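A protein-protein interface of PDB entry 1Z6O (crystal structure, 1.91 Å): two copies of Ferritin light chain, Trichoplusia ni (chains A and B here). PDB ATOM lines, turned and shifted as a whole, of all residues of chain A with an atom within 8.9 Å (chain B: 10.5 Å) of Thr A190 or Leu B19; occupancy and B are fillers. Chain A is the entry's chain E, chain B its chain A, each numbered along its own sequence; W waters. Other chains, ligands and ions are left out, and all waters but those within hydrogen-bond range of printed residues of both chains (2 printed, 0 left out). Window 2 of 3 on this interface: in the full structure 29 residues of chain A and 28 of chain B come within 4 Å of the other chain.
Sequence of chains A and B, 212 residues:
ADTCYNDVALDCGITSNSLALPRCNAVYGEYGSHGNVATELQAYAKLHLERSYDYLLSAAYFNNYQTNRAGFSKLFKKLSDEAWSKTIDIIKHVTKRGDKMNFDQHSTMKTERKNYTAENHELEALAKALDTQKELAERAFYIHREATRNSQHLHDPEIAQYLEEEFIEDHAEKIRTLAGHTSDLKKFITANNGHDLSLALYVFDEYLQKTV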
ATOM      1  N   HIS A 121     -11.956  22.616  18.877  1.00  0.00           N
ATOM      2  CA  HIS A 121     -11.931  21.172  18.721  1.00  0.00           C
ATOM      3  C   HIS A 121     -13.377  20.745  19.057  1.00  0.00           C
ATOM      4  O   HIS A 121     -14.174  21.563  19.528  1.00  0.00           O
ATOM      5  CB  HIS A 121     -10.876  20.511  19.632  1.00  0.00           C
ATOM      6  CG  HIS A 121     -11.056  20.755  21.100  1.00  0.00           C
ATOM      7  ND1 HIS A 121     -10.077  21.346  21.875  1.00  0.00           N
ATOM      8  CD2 HIS A 121     -12.036  20.380  21.959  1.00  0.00           C
ATOM      9  CE1 HIS A 121     -10.443  21.319  23.144  1.00  0.00           C
ATOM     10  NE2 HIS A 121     -11.628  20.738  23.222  1.00  0.00           N
ATOM     11  N   LEU A 123     -15.023  18.886  21.445  1.00  0.00           N
ATOM     12  CA  LEU A 123     -15.595  19.085  22.780  1.00  0.00           C
ATOM     13  C   LEU A 123     -15.819  20.576  23.061  1.00  0.00           C
ATOM     14  O   LEU A 123     -16.868  20.963  23.579  1.00  0.00           O
ATOM     15  CB  LEU A 123     -14.691  18.476  23.862  1.00  0.00           C
ATOM     16  CG  LEU A 123     -15.155  18.717  25.311  1.00  0.00           C
ATOM     17  CD1 LEU A 123     -16.561  18.150  25.526  1.00  0.00           C
ATOM     18  CD2 LEU A 123     -14.170  18.057  26.277  1.00  0.00           C
ATOM     19  N   THR A 182     -21.802  16.278  25.122  1.00  0.00           N
ATOM     20  CA  THR A 182     -20.571  16.578  25.850  1.00  0.00           C
ATOM     21  C   THR A 182     -20.209  15.434  26.781  1.00  0.00           C
ATOM     22  O   THR A 182     -19.025  15.161  26.975  1.00  0.00           O
ATOM     23  CB  THR A 182     -20.634  17.912  26.668  1.00  0.00           C
ATOM     24  OG1 THR A 182     -21.562  17.783  27.754  1.00  0.00           O
ATOM     25  CG2 THR A 182     -21.052  19.060  25.773  1.00  0.00           C
ATOM     26  N   SER A 183     -21.207  14.760  27.362  1.00  0.00           N
ATOM     27  CA  SER A 183     -20.915  13.615  28.238  1.00  0.00           C
ATOM     28  C   SER A 183     -20.270  12.489  27.432  1.00  0.00           C
ATOM     29  O   SER A 183     -19.348  11.826  27.907  1.00  0.00           O
ATOM     30  CB  SER A 183     -22.187  13.045  28.887  1.00  0.00           C
ATOM     31  OG  SER A 183     -22.760  13.980  29.767  1.00  0.00           O
ATOM     32  N   ASP A 184     -20.783  12.244  26.230  1.00  0.00           N
ATOM     33  CA  ASP A 184     -20.211  11.191  25.399  1.00  0.00           C
ATOM     34  C   ASP A 184     -18.752  11.492  25.065  1.00  0.00           C
ATOM     35  O   ASP A 184     -17.902  10.613  25.168  1.00  0.00           O
ATOM     36  CB  ASP A 184     -21.010  11.018  24.102  1.00  0.00           C
ATOM     37  CG  ASP A 184     -22.382  10.356  24.340  1.00  0.00           C
ATOM     38  OD1 ASP A 184     -22.570   9.712  25.392  1.00  0.00           O
ATOM     39  OD2 ASP A 184     -23.271  10.468  23.469  1.00  0.00           O
ATOM     40  N   LEU A 185     -18.462  12.732  24.666  1.00  0.00           N
ATOM     41  CA  LEU A 185     -17.087  13.104  24.321  1.00  0.00           C
ATOM     42  C   LEU A 185     -16.178  13.033  25.539  1.00  0.00           C
ATOM     43  O   LEU A 185     -15.034  12.592  25.447  1.00  0.00           O
ATOM     44  CB  LEU A 185     -17.028  14.518  23.737  1.00  0.00           C
ATOM     45  CG  LEU A 185     -17.609  14.803  22.348  1.00  0.00           C
ATOM     46  CD1 LEU A 185     -16.642  15.722  21.619  1.00  0.00           C
ATOM     47  CD2 LEU A 185     -17.792  13.546  21.547  1.00  0.00           C
ATOM     48  N   LYS A 186     -16.687  13.473  26.684  1.00  0.00           N
ATOM     49  CA  LYS A 186     -15.907  13.419  27.915  1.00  0.00           C
ATOM     50  C   LYS A 186     -15.464  11.975  28.183  1.00  0.00           C
ATOM     51  O   LYS A 186     -14.316  11.725  28.556  1.00  0.00           O
ATOM     52  CB  LYS A 186     -16.751  13.933  29.091  1.00  0.00           C
ATOM     53  CG  LYS A 186     -16.138  13.682  30.462  1.00  0.00           C
ATOM     54  CD  LYS A 186     -17.078  14.156  31.577  1.00  0.00           C
ATOM     55  CE  LYS A 186     -16.594  13.668  32.940  1.00  0.00           C
ATOM     56  NZ  LYS A 186     -17.402  14.223  34.066  1.00  0.00           N
ATOM     57  N   LYS A 187     -16.369  11.019  27.993  1.00  0.00           N
ATOM     58  CA  LYS A 187     -16.018   9.622  28.224  1.00  0.00           C
ATOM     59  C   LYS A 187     -14.995   9.108  27.217  1.00  0.00           C
ATOM     60  O   LYS A 187     -14.105   8.343  27.584  1.00  0.00           O
ATOM     61  CB  LYS A 187     -17.271   8.741  28.199  1.00  0.00           C
ATOM     62  CG  LYS A 187     -18.213   9.032  29.367  1.00  0.00           C
ATOM     63  CD  LYS A 187     -19.484   8.195  29.316  1.00  0.00           C
ATOM     64  CE  LYS A 187     -20.440   8.567  30.459  1.00  0.00           C
ATOM     65  NZ  LYS A 187     -21.590   7.606  30.530  1.00  0.00           N
ATOM     66  N   PHE A 188     -15.118   9.515  25.953  1.00  0.00           N
ATOM     67  CA  PHE A 188     -14.163   9.080  24.923  1.00  0.00           C
ATOM     68  C   PHE A 188     -12.769   9.578  25.294  1.00  0.00           C
ATOM     69  O   PHE A 188     -11.762   8.918  25.044  1.00  0.00           O
ATOM     70  CB  PHE A 188     -14.503   9.681  23.552  1.00  0.00           C
ATOM     71  CG  PHE A 188     -15.822   9.227  22.980  1.00  0.00           C
ATOM     72  CD1 PHE A 188     -16.539  10.070  22.136  1.00  0.00           C
ATOM     73  CD2 PHE A 188     -16.327   7.953  23.248  1.00  0.00           C
ATOM     74  CE1 PHE A 188     -17.746   9.658  21.556  1.00  0.00           C
ATOM     75  CE2 PHE A 188     -17.535   7.527  22.672  1.00  0.00           C
ATOM     76  CZ  PHE A 188     -18.242   8.385  21.826  1.00  0.00           C
ATOM     77  N   ILE A 189     -12.721  10.771  25.874  1.00  0.00           N
ATOM     78  CA  ILE A 189     -11.451  11.379  26.247  1.00  0.00           C
ATOM     79  C   ILE A 189     -10.828  10.753  27.489  1.00  0.00           C
ATOM     80  O   ILE A 189      -9.614  10.579  27.555  1.00  0.00           O
ATOM     81  CB  ILE A 189     -11.638  12.909  26.491  1.00  0.00           C
ATOM     82  CG1 ILE A 189     -11.914  13.607  25.157  1.00  0.00           C
ATOM     83  CG2 ILE A 189     -10.403  13.512  27.202  1.00  0.00           C
ATOM     84  CD1 ILE A 189     -12.487  15.021  25.309  1.00  0.00           C
ATOM     85  N   THR A 190     -11.653  10.394  28.463  1.00  0.00           N
ATOM     86  CA  THR A 190     -11.125   9.858  29.710  1.00  0.00           C
ATOM     87  C   THR A 190     -11.003   8.346  29.863  1.00  0.00           C
ATOM     88  O   THR A 190     -10.064   7.875  30.498  1.00  0.00           O
ATOM     89  CB  THR A 190     -11.937  10.390  30.911  1.00  0.00           C
ATOM     90  OG1 THR A 190     -13.278   9.897  30.843  1.00  0.00           O
ATOM     91  CG2 THR A 190     -11.976  11.914  30.891  1.00  0.00           C
ATOM     92  N   ALA A 191     -11.931   7.578  29.303  1.00  0.00           N
ATOM     93  CA  ALA A 191     -11.859   6.129  29.460  1.00  0.00           C
ATOM     94  C   ALA A 191     -10.644   5.521  28.763  1.00  0.00           C
ATOM     95  O   ALA A 191     -10.227   5.979  27.696  1.00  0.00           O
ATOM     96  CB  ALA A 191     -13.143   5.474  28.945  1.00  0.00           C
ATOM     97  N   ASN A 192     -10.066   4.497  29.389  1.00  0.00           N
ATOM     98  CA  ASN A 192      -8.913   3.799  28.830  1.00  0.00           C
ATOM     99  C   ASN A 192      -7.844   4.769  28.344  1.00  0.00           C
ATOM    100  O   ASN A 192      -7.301   4.630  27.241  1.00  0.00           O
ATOM    101  CB  ASN A 192      -9.388   2.895  27.691  1.00  0.00           C
ATOM    102  CG  ASN A 192     -10.442   1.891  28.155  1.00  0.00           C
ATOM    103  OD1 ASN A 192     -10.135   0.937  28.870  1.00  0.00           O
ATOM    104  ND2 ASN A 192     -11.686   2.120  27.772  1.00  0.00           N
ATOM    105  N   ASN A 193      -7.561   5.761  29.180  1.00  0.00           N
ATOM    106  CA  ASN A 193      -6.552   6.770  28.884  1.00  0.00           C
ATOM    107  C   ASN A 193      -6.781   7.520  27.583  1.00  0.00           C
ATOM    108  O   ASN A 193      -5.831   8.038  26.996  1.00  0.00           O
ATOM    109  CB  ASN A 193      -5.168   6.125  28.860  1.00  0.00           C
ATOM    110  CG  ASN A 193      -4.787   5.535  30.205  1.00  0.00           C
ATOM    111  OD1 ASN A 193      -4.793   6.230  31.221  1.00  0.00           O
ATOM    112  ND2 ASN A 193      -4.467   4.245  30.220  1.00  0.00           N
ATOM    113  N   GLY A 194      -8.032   7.582  27.131  1.00  0.00           N
ATOM    114  CA  GLY A 194      -8.330   8.291  25.896  1.00  0.00           C
ATOM    115  C   GLY A 194      -7.792   7.631  24.639  1.00  0.00           C
ATOM    116  O   GLY A 194      -7.733   8.261  23.580  1.00  0.00           O
ATOM    117  N   HIS A 195      -7.423   6.358  24.735  1.00  0.00           N
ATOM    118  CA  HIS A 195      -6.869   5.641  23.585  1.00  0.00           C
ATOM    119  C   HIS A 195      -7.761   5.515  22.354  1.00  0.00           C
ATOM    120  O   HIS A 195      -7.259   5.417  21.238  1.00  0.00           O
ATOM    121  CB  HIS A 195      -6.420   4.234  23.998  1.00  0.00           C
ATOM    122  CG  HIS A 195      -5.129   4.212  24.754  1.00  0.00           C
ATOM    123  ND1 HIS A 195      -4.081   5.055  24.456  1.00  0.00           N
ATOM    124  CD2 HIS A 195      -4.717   3.453  25.797  1.00  0.00           C
ATOM    125  CE1 HIS A 195      -3.079   4.820  25.285  1.00  0.00           C
ATOM    126  NE2 HIS A 195      -3.439   3.852  26.109  1.00  0.00           N
ATOM    127  N   ASP A 196      -9.072   5.489  22.542  1.00  0.00           N
ATOM    128  CA  ASP A 196      -9.964   5.355  21.399  1.00  0.00           C
ATOM    129  C   ASP A 196     -10.442   6.694  20.848  1.00  0.00           C
ATOM    130  O   ASP A 196     -11.275   6.724  19.943  1.00  0.00           O
ATOM    131  CB  ASP A 196     -11.190   4.527  21.790  1.00  0.00           C
ATOM    132  CG  ASP A 196     -10.887   3.037  21.865  1.00  0.00           C
ATOM    133  OD1 ASP A 196      -9.739   2.646  21.569  1.00  0.00           O
ATOM    134  OD2 ASP A 196     -11.796   2.259  22.214  1.00  0.00           O
ATOM    135  N   LEU A 197      -9.909   7.796  21.362  1.00  0.00           N
ATOM    136  CA  LEU A 197     -10.402   9.104  20.936  1.00  0.00           C
ATOM    137  C   LEU A 197     -10.564   9.374  19.440  1.00  0.00           C
ATOM    138  O   LEU A 197     -11.629   9.811  19.013  1.00  0.00           O
ATOM    139  CB  LEU A 197      -9.564  10.232  21.558  1.00  0.00           C
ATOM    140  CG  LEU A 197     -10.126  11.645  21.302  1.00  0.00           C
ATOM    141  CD1 LEU A 197     -11.560  11.764  21.857  1.00  0.00           C
ATOM    142  CD2 LEU A 197      -9.214  12.690  21.964  1.00  0.00           C
ATOM    143  N   CYS B   4     -19.920  25.755  30.693  1.00  0.00           N
ATOM    144  CA  CYS B   4     -19.369  24.487  30.258  1.00  0.00           C
ATOM    145  C   CYS B   4     -18.106  24.773  29.430  1.00  0.00           C
ATOM    146  O   CYS B   4     -17.094  24.081  29.557  1.00  0.00           O
ATOM    147  CB  CYS B   4     -20.429  23.725  29.446  1.00  0.00           C
ATOM    148  SG  CYS B   4     -19.795  22.253  28.581  1.00  0.00           S
ATOM    149  N   TYR B   5     -18.153  25.814  28.603  1.00  0.00           N
ATOM    150  CA  TYR B   5     -17.001  26.165  27.771  1.00  0.00           C
ATOM    151  C   TYR B   5     -15.772  26.486  28.632  1.00  0.00           C
ATOM    152  O   TYR B   5     -14.659  26.050  28.337  1.00  0.00           O
ATOM    153  CB  TYR B   5     -17.333  27.379  26.904  1.00  0.00           C
ATOM    154  CG  TYR B   5     -16.285  27.706  25.868  1.00  0.00           C
ATOM    155  CD1 TYR B   5     -16.131  26.908  24.738  1.00  0.00           C
ATOM    156  CD2 TYR B   5     -15.484  28.846  25.987  1.00  0.00           C
ATOM    157  CE1 TYR B   5     -15.218  27.235  23.741  1.00  0.00           C
ATOM    158  CE2 TYR B   5     -14.559  29.185  24.992  1.00  0.00           C
ATOM    159  CZ  TYR B   5     -14.437  28.372  23.867  1.00  0.00           C
ATOM    160  OH  TYR B   5     -13.560  28.693  22.853  1.00  0.00           O
ATOM    161  N   ASN B   6     -15.970  27.260  29.691  1.00  0.00           N
ATOM    162  CA  ASN B   6     -14.849  27.593  30.567  1.00  0.00           C
ATOM    163  C   ASN B   6     -14.322  26.342  31.281  1.00  0.00           C
ATOM    164  O   ASN B   6     -13.118  26.208  31.487  1.00  0.00           O
ATOM    165  CB  ASN B   6     -15.252  28.645  31.599  1.00  0.00           C
ATOM    166  CG  ASN B   6     -14.066  29.104  32.437  1.00  0.00           C
ATOM    167  OD1 ASN B   6     -13.060  29.577  31.896  1.00  0.00           O
ATOM    168  ND2 ASN B   6     -14.170  28.954  33.756  1.00  0.00           N
ATOM    169  N   ASP B   7     -15.210  25.426  31.664  1.00  0.00           N
ATOM    170  CA  ASP B   7     -14.762  24.186  32.313  1.00  0.00           C
ATOM    171  C   ASP B   7     -13.885  23.402  31.343  1.00  0.00           C
ATOM    172  O   ASP B   7     -12.869  22.823  31.733  1.00  0.00           O
ATOM    173  CB  ASP B   7     -15.947  23.299  32.714  1.00  0.00           C
ATOM    174  CG  ASP B   7     -16.657  23.790  33.965  1.00  0.00           C
ATOM    175  OD1 ASP B   7     -17.726  23.227  34.289  1.00  0.00           O
ATOM    176  OD2 ASP B   7     -16.153  24.726  34.626  1.00  0.00           O
ATOM    177  N   VAL B   8     -14.281  23.369  30.073  1.00  0.00           N
ATOM    178  CA  VAL B   8     -13.497  22.650  29.077  1.00  0.00           C
ATOM    179  C   VAL B   8     -12.116  23.293  28.896  1.00  0.00           C
ATOM    180  O   VAL B   8     -11.102  22.595  28.857  1.00  0.00           O
ATOM    181  CB  VAL B   8     -14.227  22.605  27.711  1.00  0.00           C
ATOM    182  CG1 VAL B   8     -13.278  22.089  26.621  1.00  0.00           C
ATOM    183  CG2 VAL B   8     -15.442  21.670  27.810  1.00  0.00           C
ATOM    184  N   ALA B   9     -12.083  24.616  28.788  1.00  0.00           N
ATOM    185  CA  ALA B   9     -10.820  25.339  28.613  1.00  0.00           C
ATOM    186  C   ALA B   9      -9.868  25.030  29.767  1.00  0.00           C
ATOM    187  O   ALA B   9      -8.684  24.786  29.553  1.00  0.00           O
ATOM    188  CB  ALA B   9     -11.080  26.848  28.535  1.00  0.00           C
ATOM    189  N   LEU B  10     -10.388  25.031  30.987  1.00  0.00           N
ATOM    190  CA  LEU B  10      -9.570  24.741  32.157  1.00  0.00           C
ATOM    191  C   LEU B  10      -9.100  23.286  32.200  1.00  0.00           C
ATOM    192  O   LEU B  10      -7.904  23.021  32.283  1.00  0.00           O
ATOM    193  CB  LEU B  10     -10.344  25.063  33.438  1.00  0.00           C
ATOM    194  CG  LEU B  10     -10.670  26.545  33.673  1.00  0.00           C
ATOM    195  CD1 LEU B  10     -11.561  26.699  34.898  1.00  0.00           C
ATOM    196  CD2 LEU B  10      -9.378  27.329  33.850  1.00  0.00           C
ATOM    197  N   ASP B  11     -10.037  22.344  32.133  1.00  0.00           N
ATOM    198  CA  ASP B  11      -9.694  20.924  32.197  1.00  0.00           C
ATOM    199  C   ASP B  11      -8.923  20.359  31.013  1.00  0.00           C
ATOM    200  O   ASP B  11      -8.199  19.379  31.167  1.00  0.00           O
ATOM    201  CB  ASP B  11     -10.955  20.085  32.424  1.00  0.00           C
ATOM    202  CG  ASP B  11     -11.448  20.151  33.859  1.00  0.00           C
ATOM    203  OD1 ASP B  11     -10.625  19.912  34.770  1.00  0.00           O
ATOM    204  OD2 ASP B  11     -12.650  20.432  34.078  1.00  0.00           O
ATOM    205  N   CYS B  12      -9.071  20.954  29.835  1.00  0.00           N
ATOM    206  CA  CYS B  12      -8.356  20.455  28.667  1.00  0.00           C
ATOM    207  C   CYS B  12      -6.967  21.080  28.561  1.00  0.00           C
ATOM    208  O   CYS B  12      -6.311  20.988  27.524  1.00  0.00           O
ATOM    209  CB  CYS B  12      -9.159  20.712  27.383  1.00  0.00           C
ATOM    210  SG  CYS B  12     -10.664  19.686  27.239  1.00  0.00           S
ATOM    211  N   GLY B  13      -6.527  21.718  29.643  1.00  0.00           N
ATOM    212  CA  GLY B  13      -5.207  22.323  29.659  1.00  0.00           C
ATOM    213  C   GLY B  13      -4.179  21.272  30.041  1.00  0.00           C
ATOM    214  O   GLY B  13      -4.476  20.375  30.831  1.00  0.00           O
ATOM    215  N   ILE B  14      -2.975  21.371  29.484  1.00  0.00           N
ATOM    216  CA  ILE B  14      -1.909  20.410  29.776  1.00  0.00           C
ATOM    217  C   ILE B  14      -1.650  20.291  31.278  1.00  0.00           C
ATOM    218  O   ILE B  14      -1.111  19.288  31.752  1.00  0.00           O
ATOM    219  CB  ILE B  14      -0.589  20.808  29.068  1.00  0.00           C
ATOM    220  CG1 ILE B  14      -0.804  20.858  27.552  1.00  0.00           C
ATOM    221  CG2 ILE B  14       0.512  19.810  29.408  1.00  0.00           C
ATOM    222  CD1 ILE B  14      -1.254  19.537  26.943  1.00  0.00           C
ATOM    223  N   THR B  15      -2.046  21.319  32.019  1.00  0.00           N
ATOM    224  CA  THR B  15      -1.869  21.352  33.466  1.00  0.00           C
ATOM    225  C   THR B  15      -2.795  20.357  34.168  1.00  0.00           C
ATOM    226  O   THR B  15      -2.433  19.777  35.193  1.00  0.00           O
ATOM    227  CB  THR B  15      -2.167  22.763  34.023  1.00  0.00           C
ATOM    228  OG1 THR B  15      -1.358  23.727  33.340  1.00  0.00           O
ATOM    229  CG2 THR B  15      -1.872  22.824  35.517  1.00  0.00           C
ATOM    230  N   SER B  16      -3.985  20.165  33.608  1.00  0.00           N
ATOM    231  CA  SER B  16      -4.976  19.264  34.186  1.00  0.00           C
ATOM    232  C   SER B  16      -4.703  17.784  33.938  1.00  0.00           C
ATOM    233  O   SER B  16      -3.987  17.409  33.007  1.00  0.00           O
ATOM    234  CB  SER B  16      -6.371  19.616  33.660  1.00  0.00           C
ATOM    235  OG  SER B  16      -7.360  18.765  34.217  1.00  0.00           O
ATOM    236  N   ASN B  17      -5.291  16.950  34.790  1.00  0.00           N
ATOM    237  CA  ASN B  17      -5.149  15.504  34.693  1.00  0.00           C
ATOM    238  C   ASN B  17      -6.511  14.857  34.921  1.00  0.00           C
ATOM    239  O   ASN B  17      -6.609  13.681  35.277  1.00  0.00           O
ATOM    240  CB  ASN B  17      -4.147  15.005  35.734  1.00  0.00           C
ATOM    241  CG  ASN B  17      -2.792  15.678  35.604  1.00  0.00           C
ATOM    242  OD1 ASN B  17      -2.150  15.611  34.553  1.00  0.00           O
ATOM    243  ND2 ASN B  17      -2.353  16.336  36.672  1.00  0.00           N
ATOM    244  N   SER B  18      -7.562  15.645  34.717  1.00  0.00           N
ATOM    245  CA  SER B  18      -8.930  15.176  34.886  1.00  0.00           C
ATOM    246  C   SER B  18      -9.844  15.948  33.940  1.00  0.00           C
ATOM    247  O   SER B  18      -9.406  16.877  33.258  1.00  0.00           O
ATOM    248  CB  SER B  18      -9.390  15.391  36.328  1.00  0.00           C
ATOM    249  OG  SER B  18      -9.387  16.772  36.656  1.00  0.00           O
ATOM    250  N   LEU B  19     -11.113  15.562  33.902  1.00  0.00           N
ATOM    251  CA  LEU B  19     -12.079  16.230  33.043  1.00  0.00           C
ATOM    252  C   LEU B  19     -13.438  16.173  33.733  1.00  0.00           C
ATOM    253  O   LEU B  19     -14.345  15.470  33.288  1.00  0.00           O
ATOM    254  CB  LEU B  19     -12.125  15.529  31.677  1.00  0.00           C
ATOM    255  CG  LEU B  19     -12.690  16.329  30.502  1.00  0.00           C
ATOM    256  CD1 LEU B  19     -11.823  17.552  30.274  1.00  0.00           C
ATOM    257  CD2 LEU B  19     -12.737  15.469  29.240  1.00  0.00           C
ATOM    258  N   ALA B  20     -13.581  16.925  34.820  1.00  0.00           N
ATOM    259  CA  ALA B  20     -14.825  16.936  35.589  1.00  0.00           C
ATOM    260  C   ALA B  20     -16.018  17.546  34.845  1.00  0.00           C
ATOM    261  O   ALA B  20     -17.106  16.961  34.811  1.00  0.00           O
ATOM    262  CB  ALA B  20     -14.601  17.667  36.910  1.00  0.00           C
ATOM    263  N   LEU B  21     -15.806  18.723  34.265  1.00  0.00           N
ATOM    264  CA  LEU B  21     -16.842  19.436  33.513  1.00  0.00           C
ATOM    265  C   LEU B  21     -18.180  19.518  34.253  1.00  0.00           C
ATOM    266  O   LEU B  21     -19.223  19.146  33.716  1.00  0.00           O
ATOM    267  CB  LEU B  21     -17.051  18.768  32.147  1.00  0.00           C
ATOM    268  CG  LEU B  21     -15.781  18.572  31.310  1.00  0.00           C
ATOM    269  CD1 LEU B  21     -16.167  18.011  29.946  1.00  0.00           C
ATOM    270  CD2 LEU B  21     -15.037  19.894  31.147  1.00  0.00           C
ATOM    271  N   PRO B  22     -18.170  20.037  35.489  1.00  0.00           N
ATOM    272  CA  PRO B  22     -19.412  20.145  36.262  1.00  0.00           C
ATOM    273  C   PRO B  22     -20.527  20.968  35.614  1.00  0.00           C
ATOM    274  O   PRO B  22     -21.702  20.695  35.844  1.00  0.00           O
ATOM    275  CB  PRO B  22     -18.940  20.727  37.601  1.00  0.00           C
ATOM    276  CG  PRO B  22     -17.727  21.521  37.224  1.00  0.00           C
ATOM    277  CD  PRO B  22     -17.033  20.619  36.225  1.00  0.00           C
ATOM    278  N   ARG B  23     -20.179  21.963  34.801  1.00  0.00           N
ATOM    279  CA  ARG B  23     -21.206  22.774  34.154  1.00  0.00           C
ATOM    280  C   ARG B  23     -21.693  22.222  32.819  1.00  0.00           C
ATOM    281  O   ARG B  23     -22.568  22.810  32.183  1.00  0.00           O
ATOM    282  CB  ARG B  23     -20.723  24.211  33.953  1.00  0.00           C
ATOM    283  CG  ARG B  23     -21.190  25.162  35.052  1.00  0.00           C
ATOM    284  CD  ARG B  23     -20.609  24.773  36.399  1.00  0.00           C
ATOM    285  NE  ARG B  23     -19.151  24.831  36.367  1.00  0.00           N
ATOM    286  CZ  ARG B  23     -18.372  24.841  37.446  1.00  0.00           C
ATOM    287  NH1 ARG B  23     -18.908  24.796  38.661  1.00  0.00           N
ATOM    288  NH2 ARG B  23     -17.052  24.905  37.307  1.00  0.00           N
ATOM    289  N   CYS B  24     -21.126  21.105  32.382  1.00  0.00           N
ATOM    290  CA  CYS B  24     -21.562  20.527  31.119  1.00  0.00           C
ATOM    291  C   CYS B  24     -22.639  19.489  31.422  1.00  0.00           C
ATOM    292  O   CYS B  24     -22.394  18.285  31.424  1.00  0.00           O
ATOM    293  CB  CYS B  24     -20.384  19.879  30.397  1.00  0.00           C
ATOM    294  SG  CYS B  24     -19.031  21.049  30.014  1.00  0.00           S
HETATM  295  O   HOH W   1     -20.857  16.253  30.353  1.00  0.00           O
HETATM  296  O   HOH W   2     -24.115  16.071  30.680  1.00  0.00           O
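Water W2 bridges OG of Ser A183 and O of Cys B24.
Water W1 lies within hydrogen-bond range of the backbone carbonyl oxygen (O) of Cys B24, the side-chain hydroxyl (OG) of Ser A183 and the side-chain hydroxyl (OG1) of Thr A182.
The side-chain amino group (NZ) of Lys A186 sits at hydrogen-bond distance from the backbone carbonyl oxygen (O) of Ala B20.
The backbone carbonyl oxygen (O) of Leu B19 lies close to the side-chain amino group (NZ) of Lys A186 (3.4 Å).
Thr A190 touches just one residue of chain B: Leu B19 (3.7 Å).
Lys A186 touches just these residues of chain B: Leu B19 and Ala B20.
No residue of chain B comes within 4 Å of Ala A191.
Ser B18 touches none of the printed residues of chain A.
Ala B20 touches one residue of chain A.
Of the printed residues of chain A, Cys B24 touches Thr A182 (3.6 Å).
Printed residues of chain A within 4 Å of Val B8: Leu A123 (3.9 Å).
Of the printed residues of chain B, Thr A182 touches Cys B24.
Printed residues of chain A within 4 Å of Cys B12: Leu A123 (3.98 Å).
Of the printed residues of chain B, Leu A123 touches Val B8 and Cys B12.
Ala B9 touches none of the printed residues of chain A.
Ser B16 touches none of the printed residues of chain A.
The nearest printed residue of chain B that does not touch Thr A182 is Cys B4 (4.4 Å).
No position is printed for both chains.
Of the 7 pairs that touch across the chains among the printed residues, none has its exchanged pair printed and touching as well.
Hydrophobic or aromatic side chains of chain A that line the printed part of chain B: Leu A123 and Ile A189.
Along chain A the printed residues that touch a printed residue of chain B span positions 123 to 190.
Of the 21 printed residues of chain B, 5 touch a printed residue of chain A.
Among the printed residues, no Asp or Glu carboxylate lies within 4 Å of a Lys or Arg side-chain nitrogen of the other chain.
Among the printed residues, merely in contact across the chains: Thr A182 with Cys B24, Ile A189 with Leu B19, Thr A190 with Leu B19, Leu A123 with Val B8 and Leu A123 with Cys B12.
The backbone carbonyl oxygen (O) of Lys A186 lies within hydrogen-bond range of the side-chain hydroxyl (OG1) of Thr A190 (3.1 Å).
SG of Cys B4 is disulfide-bonded to SG of Cys B24, 2.0 Å away.
The backbone carbonyl oxygen (O) of Ile A189 lies close to the backbone NH (N) of Gly A194, 3.4 Å away.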
